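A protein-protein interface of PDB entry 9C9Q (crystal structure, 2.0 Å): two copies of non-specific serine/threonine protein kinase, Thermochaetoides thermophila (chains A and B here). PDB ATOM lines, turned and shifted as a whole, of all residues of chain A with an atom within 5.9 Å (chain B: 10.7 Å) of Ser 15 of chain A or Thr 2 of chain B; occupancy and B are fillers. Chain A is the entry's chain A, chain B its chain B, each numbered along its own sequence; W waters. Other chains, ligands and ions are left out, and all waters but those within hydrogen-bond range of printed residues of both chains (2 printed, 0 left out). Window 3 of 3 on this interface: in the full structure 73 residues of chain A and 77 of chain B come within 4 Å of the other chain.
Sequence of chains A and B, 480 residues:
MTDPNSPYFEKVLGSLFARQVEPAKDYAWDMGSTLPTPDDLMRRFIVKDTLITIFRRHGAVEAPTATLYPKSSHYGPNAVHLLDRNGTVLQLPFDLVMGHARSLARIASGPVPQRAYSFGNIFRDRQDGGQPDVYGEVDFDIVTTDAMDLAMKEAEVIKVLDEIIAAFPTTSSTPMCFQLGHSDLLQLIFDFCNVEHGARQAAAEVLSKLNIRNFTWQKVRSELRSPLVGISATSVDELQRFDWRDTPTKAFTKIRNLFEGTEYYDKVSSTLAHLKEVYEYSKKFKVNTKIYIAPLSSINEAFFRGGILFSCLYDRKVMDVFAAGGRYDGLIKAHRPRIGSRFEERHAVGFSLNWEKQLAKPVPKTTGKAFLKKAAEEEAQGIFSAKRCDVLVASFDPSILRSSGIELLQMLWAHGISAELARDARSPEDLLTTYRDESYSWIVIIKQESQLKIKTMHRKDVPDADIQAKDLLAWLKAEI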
ATOM      1  N   GLU A  10     -27.685  22.385   9.926  1.00  0.00           N
ATOM      2  CA  GLU A  10     -28.655  23.253   9.261  1.00  0.00           C
ATOM      3  C   GLU A  10     -28.119  24.672   9.132  1.00  0.00           C
ATOM      4  O   GLU A  10     -28.051  25.220   8.027  1.00  0.00           O
ATOM      5  CB  GLU A  10     -29.985  23.269  10.014  1.00  0.00           C
ATOM      6  CG  GLU A  10     -31.228  23.593   9.151  1.00  0.00           C
ATOM      7  CD  GLU A  10     -31.145  24.896   8.351  1.00  0.00           C
ATOM      8  OE1 GLU A  10     -31.387  24.870   7.123  1.00  0.00           O
ATOM      9  OE2 GLU A  10     -30.843  25.956   8.937  1.00  0.00           O
ATOM     10  N   LYS A  11     -27.748  25.289  10.262  1.00  0.00           N
ATOM     11  CA  LYS A  11     -27.397  26.706  10.258  1.00  0.00           C
ATOM     12  C   LYS A  11     -26.293  27.002   9.245  1.00  0.00           C
ATOM     13  O   LYS A  11     -26.363  27.997   8.515  1.00  0.00           O
ATOM     14  CB  LYS A  11     -26.988  27.160  11.668  1.00  0.00           C
ATOM     15  CG  LYS A  11     -27.676  28.461  12.119  1.00  0.00           C
ATOM     16  CD  LYS A  11     -27.142  29.015  13.459  1.00  0.00           C
ATOM     17  CE  LYS A  11     -27.967  28.557  14.670  1.00  0.00           C
ATOM     18  NZ  LYS A  11     -27.451  29.117  15.970  1.00  0.00           N
ATOM     19  N   VAL A  12     -25.286  26.135   9.166  1.00  0.00           N
ATOM     20  CA  VAL A  12     -24.230  26.320   8.177  1.00  0.00           C
ATOM     21  C   VAL A  12     -24.775  26.124   6.765  1.00  0.00           C
ATOM     22  O   VAL A  12     -24.367  26.815   5.820  1.00  0.00           O
ATOM     23  CB  VAL A  12     -23.064  25.362   8.460  1.00  0.00           C
ATOM     24  CG1 VAL A  12     -21.911  25.669   7.528  1.00  0.00           C
ATOM     25  CG2 VAL A  12     -22.632  25.456   9.922  1.00  0.00           C
ATOM     26  N   LEU A  13     -25.688  25.166   6.596  1.00  0.00           N
ATOM     27  CA  LEU A  13     -26.289  24.920   5.293  1.00  0.00           C
ATOM     28  C   LEU A  13     -27.027  26.156   4.792  1.00  0.00           C
ATOM     29  O   LEU A  13     -26.778  26.634   3.679  1.00  0.00           O
ATOM     30  CB  LEU A  13     -27.230  23.719   5.386  1.00  0.00           C
ATOM     31  CG  LEU A  13     -27.471  22.939   4.109  1.00  0.00           C
ATOM     32  CD1 LEU A  13     -26.134  22.615   3.472  1.00  0.00           C
ATOM     33  CD2 LEU A  13     -28.243  21.677   4.436  1.00  0.00           C
ATOM     34  N   GLY A  14     -27.928  26.701   5.614  1.00  0.00           N
ATOM     35  CA  GLY A  14     -28.642  27.903   5.217  1.00  0.00           C
ATOM     36  C   GLY A  14     -27.719  29.067   4.917  1.00  0.00           C
ATOM     37  O   GLY A  14     -28.016  29.892   4.050  1.00  0.00           O
ATOM     38  N   SER A  15     -26.581  29.140   5.609  1.00  0.00           N
ATOM     39  CA  SER A  15     -25.626  30.210   5.348  1.00  0.00           C
ATOM     40  C   SER A  15     -24.813  29.950   4.086  1.00  0.00           C
ATOM     41  O   SER A  15     -24.459  30.901   3.365  1.00  0.00           O
ATOM     42  CB  SER A  15     -24.696  30.372   6.545  1.00  0.00           C
ATOM     43  OG  SER A  15     -24.111  31.661   6.557  1.00  0.00           O
ATOM     44  N   LEU A  16     -24.502  28.679   3.818  1.00  0.00           N
ATOM     45  CA  LEU A  16     -23.884  28.308   2.549  1.00  0.00           C
ATOM     46  C   LEU A  16     -24.730  28.753   1.363  1.00  0.00           C
ATOM     47  O   LEU A  16     -24.204  29.301   0.390  1.00  0.00           O
ATOM     48  CB  LEU A  16     -23.663  26.803   2.494  1.00  0.00           C
ATOM     49  CG  LEU A  16     -22.379  26.282   3.140  1.00  0.00           C
ATOM     50  CD1 LEU A  16     -22.506  24.799   3.358  1.00  0.00           C
ATOM     51  CD2 LEU A  16     -21.169  26.581   2.285  1.00  0.00           C
ATOM     52  N   PHE A  17     -26.040  28.524   1.420  1.00  0.00           N
ATOM     53  CA  PHE A  17     -26.900  28.861   0.293  1.00  0.00           C
ATOM     54  C   PHE A  17     -27.149  30.352   0.181  1.00  0.00           C
ATOM     55  O   PHE A  17     -27.647  30.811  -0.854  1.00  0.00           O
ATOM     56  CB  PHE A  17     -28.236  28.120   0.393  1.00  0.00           C
ATOM     57  CG  PHE A  17     -28.201  26.742  -0.215  1.00  0.00           C
ATOM     58  CD1 PHE A  17     -28.447  26.563  -1.565  1.00  0.00           C
ATOM     59  CD2 PHE A  17     -27.886  25.642   0.556  1.00  0.00           C
ATOM     60  CE1 PHE A  17     -28.399  25.296  -2.139  1.00  0.00           C
ATOM     61  CE2 PHE A  17     -27.832  24.372  -0.006  1.00  0.00           C
ATOM     62  CZ  PHE A  17     -28.093  24.194  -1.353  1.00  0.00           C
ATOM     63  N   ALA A  18     -26.805  31.112   1.213  1.00  0.00           N
ATOM     64  CA  ALA A  18     -26.906  32.560   1.171  1.00  0.00           C
ATOM     65  C   ALA A  18     -25.634  33.220   0.657  1.00  0.00           C
ATOM     66  O   ALA A  18     -25.655  34.411   0.329  1.00  0.00           O
ATOM     67  CB  ALA A  18     -27.236  33.091   2.570  1.00  0.00           C
ATOM     68  N   ARG A  19     -24.542  32.476   0.562  1.00  0.00           N
ATOM     69  CA  ARG A  19     -23.258  33.068   0.235  1.00  0.00           C
ATOM     70  C   ARG A  19     -23.199  33.502  -1.224  1.00  0.00           C
ATOM     71  O   ARG A  19     -23.647  32.790  -2.127  1.00  0.00           O
ATOM     72  CB  ARG A  19     -22.144  32.079   0.535  1.00  0.00           C
ATOM     73  CG  ARG A  19     -20.768  32.656   0.360  1.00  0.00           C
ATOM     74  CD  ARG A  19     -19.788  31.941   1.251  1.00  0.00           C
ATOM     75  NE  ARG A  19     -19.791  30.511   0.976  1.00  0.00           N
ATOM     76  CZ  ARG A  19     -18.749  29.718   1.173  1.00  0.00           C
ATOM     77  NH1 ARG A  19     -17.614  30.181   1.673  1.00  0.00           N
ATOM     78  NH2 ARG A  19     -18.844  28.432   0.845  1.00  0.00           N
ATOM     79  N   MET B   1     -23.945  38.929   6.928  1.00  0.00           N
ATOM     80  CA  MET B   1     -22.883  39.520   7.746  1.00  0.00           C
ATOM     81  C   MET B   1     -21.810  38.504   8.142  1.00  0.00           C
ATOM     82  O   MET B   1     -20.741  38.882   8.622  1.00  0.00           O
ATOM     83  CB  MET B   1     -23.469  40.163   9.002  1.00  0.00           C
ATOM     84  CG  MET B   1     -23.661  41.658   8.876  1.00  0.00           C
ATOM     85  SD  MET B   1     -24.888  42.294  10.035  1.00  0.00           S
ATOM     86  CE  MET B   1     -24.570  44.059   9.926  1.00  0.00           C
ATOM     87  N   THR B   2     -22.104  37.220   7.945  1.00  0.00           N
ATOM     88  CA  THR B   2     -21.109  36.182   8.174  1.00  0.00           C
ATOM     89  C   THR B   2     -19.881  36.418   7.297  1.00  0.00           C
ATOM     90  O   THR B   2     -19.983  36.895   6.162  1.00  0.00           O
ATOM     91  CB  THR B   2     -21.706  34.797   7.875  1.00  0.00           C
ATOM     92  OG1 THR B   2     -22.983  34.663   8.516  1.00  0.00           O
ATOM     93  CG2 THR B   2     -20.789  33.686   8.371  1.00  0.00           C
ATOM     94  N   ASP B   3     -18.710  36.097   7.845  1.00  0.00           N
ATOM     95  CA  ASP B   3     -17.478  36.042   7.064  1.00  0.00           C
ATOM     96  C   ASP B   3     -17.589  34.977   5.973  1.00  0.00           C
ATOM     97  O   ASP B   3     -17.694  33.781   6.296  1.00  0.00           O
ATOM     98  CB  ASP B   3     -16.290  35.734   7.975  1.00  0.00           C
ATOM     99  CG  ASP B   3     -14.978  35.611   7.212  1.00  0.00           C
ATOM    100  OD1 ASP B   3     -14.908  36.048   6.042  1.00  0.00           O
ATOM    101  OD2 ASP B   3     -14.010  35.076   7.786  1.00  0.00           O
ATOM    102  N   PRO B   4     -17.553  35.355   4.687  1.00  0.00           N
ATOM    103  CA  PRO B   4     -17.657  34.347   3.614  1.00  0.00           C
ATOM    104  C   PRO B   4     -16.545  33.322   3.630  1.00  0.00           C
ATOM    105  O   PRO B   4     -16.726  32.224   3.095  1.00  0.00           O
ATOM    106  CB  PRO B   4     -17.602  35.187   2.330  1.00  0.00           C
ATOM    107  CG  PRO B   4     -17.956  36.582   2.756  1.00  0.00           C
ATOM    108  CD  PRO B   4     -17.442  36.724   4.153  1.00  0.00           C
ATOM    109  N   ASN B   5     -15.395  33.640   4.215  1.00  0.00           N
ATOM    110  CA  ASN B   5     -14.275  32.715   4.266  1.00  0.00           C
ATOM    111  C   ASN B   5     -14.203  31.979   5.595  1.00  0.00           C
ATOM    112  O   ASN B   5     -13.144  31.450   5.949  1.00  0.00           O
ATOM    113  CB  ASN B   5     -12.971  33.464   3.984  1.00  0.00           C
ATOM    114  CG  ASN B   5     -13.059  34.336   2.739  1.00  0.00           C
ATOM    115  OD1 ASN B   5     -12.890  35.557   2.803  1.00  0.00           O
ATOM    116  ND2 ASN B   5     -13.342  33.711   1.598  1.00  0.00           N
ATOM    117  N   SER B   6     -15.308  31.940   6.337  1.00  0.00           N
ATOM    118  CA  SER B   6     -15.337  31.235   7.612  1.00  0.00           C
ATOM    119  C   SER B   6     -15.040  29.747   7.411  1.00  0.00           C
ATOM    120  O   SER B   6     -15.651  29.107   6.544  1.00  0.00           O
ATOM    121  CB  SER B   6     -16.698  31.422   8.280  1.00  0.00           C
ATOM    122  OG  SER B   6     -16.759  30.710   9.502  1.00  0.00           O
ATOM    123  N   PRO B   7     -14.127  29.159   8.195  1.00  0.00           N
ATOM    124  CA  PRO B   7     -13.714  27.764   7.947  1.00  0.00           C
ATOM    125  C   PRO B   7     -14.785  26.730   8.267  1.00  0.00           C
ATOM    126  O   PRO B   7     -14.593  25.548   7.945  1.00  0.00           O
ATOM    127  CB  PRO B   7     -12.490  27.586   8.862  1.00  0.00           C
ATOM    128  CG  PRO B   7     -12.131  28.986   9.353  1.00  0.00           C
ATOM    129  CD  PRO B   7     -13.412  29.753   9.336  1.00  0.00           C
ATOM    130  N   TYR B   8     -15.883  27.121   8.916  1.00  0.00           N
ATOM    131  CA  TYR B   8     -16.998  26.198   9.100  1.00  0.00           C
ATOM    132  C   TYR B   8     -17.654  25.864   7.767  1.00  0.00           C
ATOM    133  O   TYR B   8     -18.277  24.804   7.630  1.00  0.00           O
ATOM    134  CB  TYR B   8     -18.028  26.796  10.067  1.00  0.00           C
ATOM    135  CG  TYR B   8     -17.523  27.004  11.486  1.00  0.00           C
ATOM    136  CD1 TYR B   8     -17.889  26.131  12.511  1.00  0.00           C
ATOM    137  CD2 TYR B   8     -16.685  28.077  11.803  1.00  0.00           C
ATOM    138  CE1 TYR B   8     -17.432  26.313  13.811  1.00  0.00           C
ATOM    139  CE2 TYR B   8     -16.220  28.270  13.103  1.00  0.00           C
ATOM    140  CZ  TYR B   8     -16.600  27.381  14.103  1.00  0.00           C
ATOM    141  OH  TYR B   8     -16.144  27.559  15.394  1.00  0.00           O
ATOM    142  N   PHE B   9     -17.517  26.748   6.775  1.00  0.00           N
ATOM    143  CA  PHE B   9     -18.141  26.517   5.475  1.00  0.00           C
ATOM    144  C   PHE B   9     -17.515  25.318   4.767  1.00  0.00           C
ATOM    145  O   PHE B   9     -18.226  24.400   4.338  1.00  0.00           O
ATOM    146  CB  PHE B   9     -18.051  27.786   4.625  1.00  0.00           C
ATOM    147  CG  PHE B   9     -19.128  28.800   4.936  1.00  0.00           C
ATOM    148  CD1 PHE B   9     -20.423  28.390   5.209  1.00  0.00           C
ATOM    149  CD2 PHE B   9     -18.848  30.163   4.964  1.00  0.00           C
ATOM    150  CE1 PHE B   9     -21.426  29.310   5.491  1.00  0.00           C
ATOM    151  CE2 PHE B   9     -19.844  31.091   5.254  1.00  0.00           C
ATOM    152  CZ  PHE B   9     -21.134  30.663   5.518  1.00  0.00           C
ATOM    153  N   GLU B  10     -16.183  25.286   4.661  1.00  0.00           N
ATOM    154  CA  GLU B  10     -15.537  24.114   4.075  1.00  0.00           C
ATOM    155  C   GLU B  10     -15.771  22.851   4.906  1.00  0.00           C
ATOM    156  O   GLU B  10     -15.901  21.756   4.344  1.00  0.00           O
ATOM    157  CB  GLU B  10     -14.042  24.361   3.904  1.00  0.00           C
ATOM    158  CG  GLU B  10     -13.226  23.093   3.683  1.00  0.00           C
ATOM    159  CD  GLU B  10     -13.593  22.376   2.393  1.00  0.00           C
ATOM    160  OE1 GLU B  10     -14.143  23.037   1.486  1.00  0.00           O
ATOM    161  OE2 GLU B  10     -13.336  21.154   2.285  1.00  0.00           O
ATOM    162  N   VAL B  12     -18.414  21.829   6.625  1.00  0.00           N
ATOM    163  CA  VAL B  12     -19.721  21.225   6.393  1.00  0.00           C
ATOM    164  C   VAL B  12     -19.857  20.721   4.956  1.00  0.00           C
ATOM    165  O   VAL B  12     -20.532  19.711   4.706  1.00  0.00           O
ATOM    166  CB  VAL B  12     -20.818  22.238   6.769  1.00  0.00           C
ATOM    167  CG1 VAL B  12     -22.173  21.816   6.230  1.00  0.00           C
ATOM    168  CG2 VAL B  12     -20.880  22.390   8.281  1.00  0.00           C
ATOM    169  N   LEU B  13     -19.222  21.397   3.991  1.00  0.00           N
ATOM    170  CA  LEU B  13     -19.286  20.948   2.603  1.00  0.00           C
ATOM    171  C   LEU B  13     -18.699  19.551   2.462  1.00  0.00           C
ATOM    172  O   LEU B  13     -19.396  18.607   2.074  1.00  0.00           O
ATOM    173  CB  LEU B  13     -18.550  21.928   1.685  1.00  0.00           C
ATOM    174  CG  LEU B  13     -19.296  23.185   1.257  1.00  0.00           C
ATOM    175  CD1 LEU B  13     -18.368  24.072   0.438  1.00  0.00           C
ATOM    176  CD2 LEU B  13     -20.545  22.819   0.464  1.00  0.00           C
ATOM    177  N   LEU B  16     -20.823  17.023   4.146  1.00  0.00           N
ATOM    178  CA  LEU B  16     -22.106  16.662   3.553  1.00  0.00           C
ATOM    179  C   LEU B  16     -21.943  15.935   2.221  1.00  0.00           C
ATOM    180  O   LEU B  16     -22.695  14.994   1.943  1.00  0.00           O
ATOM    181  CB  LEU B  16     -22.984  17.902   3.408  1.00  0.00           C
ATOM    182  CG  LEU B  16     -23.629  18.319   4.734  1.00  0.00           C
ATOM    183  CD1 LEU B  16     -24.425  19.598   4.585  1.00  0.00           C
ATOM    184  CD2 LEU B  16     -24.507  17.194   5.294  1.00  0.00           C
ATOM    185  N   LYS B  71     -26.264  31.133  -9.449  1.00  0.00           N
ATOM    186  CA  LYS B  71     -27.587  31.696  -9.197  1.00  0.00           C
ATOM    187  C   LYS B  71     -27.643  33.175  -9.572  1.00  0.00           C
ATOM    188  O   LYS B  71     -26.677  33.923  -9.395  1.00  0.00           O
ATOM    189  CB  LYS B  71     -27.970  31.527  -7.720  1.00  0.00           C
ATOM    190  CG  LYS B  71     -27.128  32.362  -6.750  1.00  0.00           C
ATOM    191  CD  LYS B  71     -27.899  32.708  -5.473  1.00  0.00           C
ATOM    192  CE  LYS B  71     -27.115  33.680  -4.576  1.00  0.00           C
ATOM    193  NZ  LYS B  71     -26.167  32.981  -3.641  1.00  0.00           N
ATOM    194  N   LEU B  83     -25.686  23.528  -4.534  1.00  0.00           N
ATOM    195  CA  LEU B  83     -24.305  23.867  -4.202  1.00  0.00           C
ATOM    196  C   LEU B  83     -23.358  22.884  -4.870  1.00  0.00           C
ATOM    197  O   LEU B  83     -23.541  21.673  -4.735  1.00  0.00           O
ATOM    198  CB  LEU B  83     -24.066  23.791  -2.690  1.00  0.00           C
ATOM    199  CG  LEU B  83     -24.447  24.914  -1.731  1.00  0.00           C
ATOM    200  CD1 LEU B  83     -24.155  24.434  -0.308  1.00  0.00           C
ATOM    201  CD2 LEU B  83     -23.676  26.177  -2.026  1.00  0.00           C
ATOM    202  N   GLY B  87     -18.508  25.183  -3.184  1.00  0.00           N
ATOM    203  CA  GLY B  87     -19.349  26.113  -2.464  1.00  0.00           C
ATOM    204  C   GLY B  87     -20.103  27.136  -3.284  1.00  0.00           C
ATOM    205  O   GLY B  87     -20.829  27.949  -2.696  1.00  0.00           O
ATOM    206  N   THR B  88     -19.959  27.141  -4.611  1.00  0.00           N
ATOM    207  CA  THR B  88     -20.693  28.100  -5.435  1.00  0.00           C
ATOM    208  C   THR B  88     -22.173  27.755  -5.422  1.00  0.00           C
ATOM    209  O   THR B  88     -22.546  26.598  -5.627  1.00  0.00           O
ATOM    210  CB  THR B  88     -20.183  28.080  -6.877  1.00  0.00           C
ATOM    211  OG1 THR B  88     -18.777  28.332  -6.908  1.00  0.00           O
ATOM    212  CG2 THR B  88     -20.916  29.135  -7.722  1.00  0.00           C
ATOM    213  N   VAL B  89     -23.029  28.748  -5.215  1.00  0.00           N
ATOM    214  CA  VAL B  89     -24.460  28.488  -5.307  1.00  0.00           C
ATOM    215  C   VAL B  89     -24.878  28.568  -6.769  1.00  0.00           C
ATOM    216  O   VAL B  89     -24.700  29.600  -7.427  1.00  0.00           O
ATOM    217  CB  VAL B  89     -25.279  29.452  -4.449  1.00  0.00           C
ATOM    218  CG1 VAL B  89     -26.747  29.073  -4.558  1.00  0.00           C
ATOM    219  CG2 VAL B  89     -24.810  29.412  -2.990  1.00  0.00           C
HETATM  220  O   HOH W   1     -22.432  31.371  -4.539  1.00  0.00           O
HETATM  221  O   HOH W   2     -21.946  28.792  -0.433  1.00  0.00           O
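O of Arg 19 of chain A sits at hydrogen-bond distance from NZ of Lys 71 of chain B, at 2.9 Å.
The backbone carbonyl oxygen (O) of Pro 4 of chain B sits at hydrogen-bond distance from the guanidinium group (NH1) of Arg 19 of chain A.
O of Val 89 of chain B is in hydrogen-bond range of N of Lys 71 of chain B (3.0 Å).
Among the printed residues, pairs that only touch across the chains: Ser 15 of chain A with Phe 9 of chain B, Leu 16 of chain A with Val 89 of chain B, Arg 19 of chain A with Phe 9 of chain B, Leu 16 of chain A with Phe 9 of chain B, Val 12 of chain A with Val 12 of chain B, Leu 13 of chain A with Leu 16 of chain B, Arg 19 of chain A with Val 89 of chain B, Phe 17 of chain A with Leu 83 of chain B, Leu 16 of chain A with Leu 83 of chain B, Val 12 of chain A with Tyr 8 of chain B, Ser 15 of chain A with Thr 2 of chain B, Phe 17 of chain A with Val 89 of chain B, Phe 17 of chain A with Lys 71 of chain B and Val 12 of chain A with Phe 9 of chain B.
Ser 15 of chain A touches just these residues of chain B: Thr 2 and Phe 9.
Val 12 of chain A touches just these residues of chain B: Tyr 8, Phe 9 and Val 12.
Printed residues of chain A within 4 Å of Pro 4 of chain B: Arg 19.
Printed residues of chain A within 4 Å of Val 12 of chain B: Val 12.
The nearest residue of chain B that does not touch Ser 15 of chain A is Val 89 of chain B (6.5 Å).
The nearest printed residue of chain A that does not touch Thr 2 of chain B is Arg 19 of chain A (7.0 Å).
The nearest printed residue of chain B that does not touch Leu 13 of chain A is Leu 83 of chain B (4.6 Å).
Printed residues of chain A that touch a printed residue of chain B: Val 12, Leu 13, Ser 15, Leu 16, Phe 17 and Arg 19.
Among the printed residues, no Asp or Glu carboxylate lies within 4 Å of a Lys or Arg side-chain nitrogen of the other chain.
Val 12 of chain B touches its own counterpart, Val 12 of chain A.
Leu 13 of chain A touches Leu 16 of chain B, but with the chains exchanged Leu 16 of chain A does not touch Leu 13 of chain B (4.01 Å).
Of the 16 pairs that touch across the chains among the printed residues, 1 has its exchanged pair printed and touching as well.
Water W2 lies within hydrogen-bond range of the backbone carbonyl oxygen of Leu 16 of chain A (2.5 Å), the backbone carbonyl oxygen of Gly 87 of chain B (2.7 Å) and the guanidinium group of Arg 19 of chain A (3.1 Å).
Water W1 bridges N of Val 89 of chain B (2.8 Å) and O of Arg 19 of chain A (3.1 Å).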
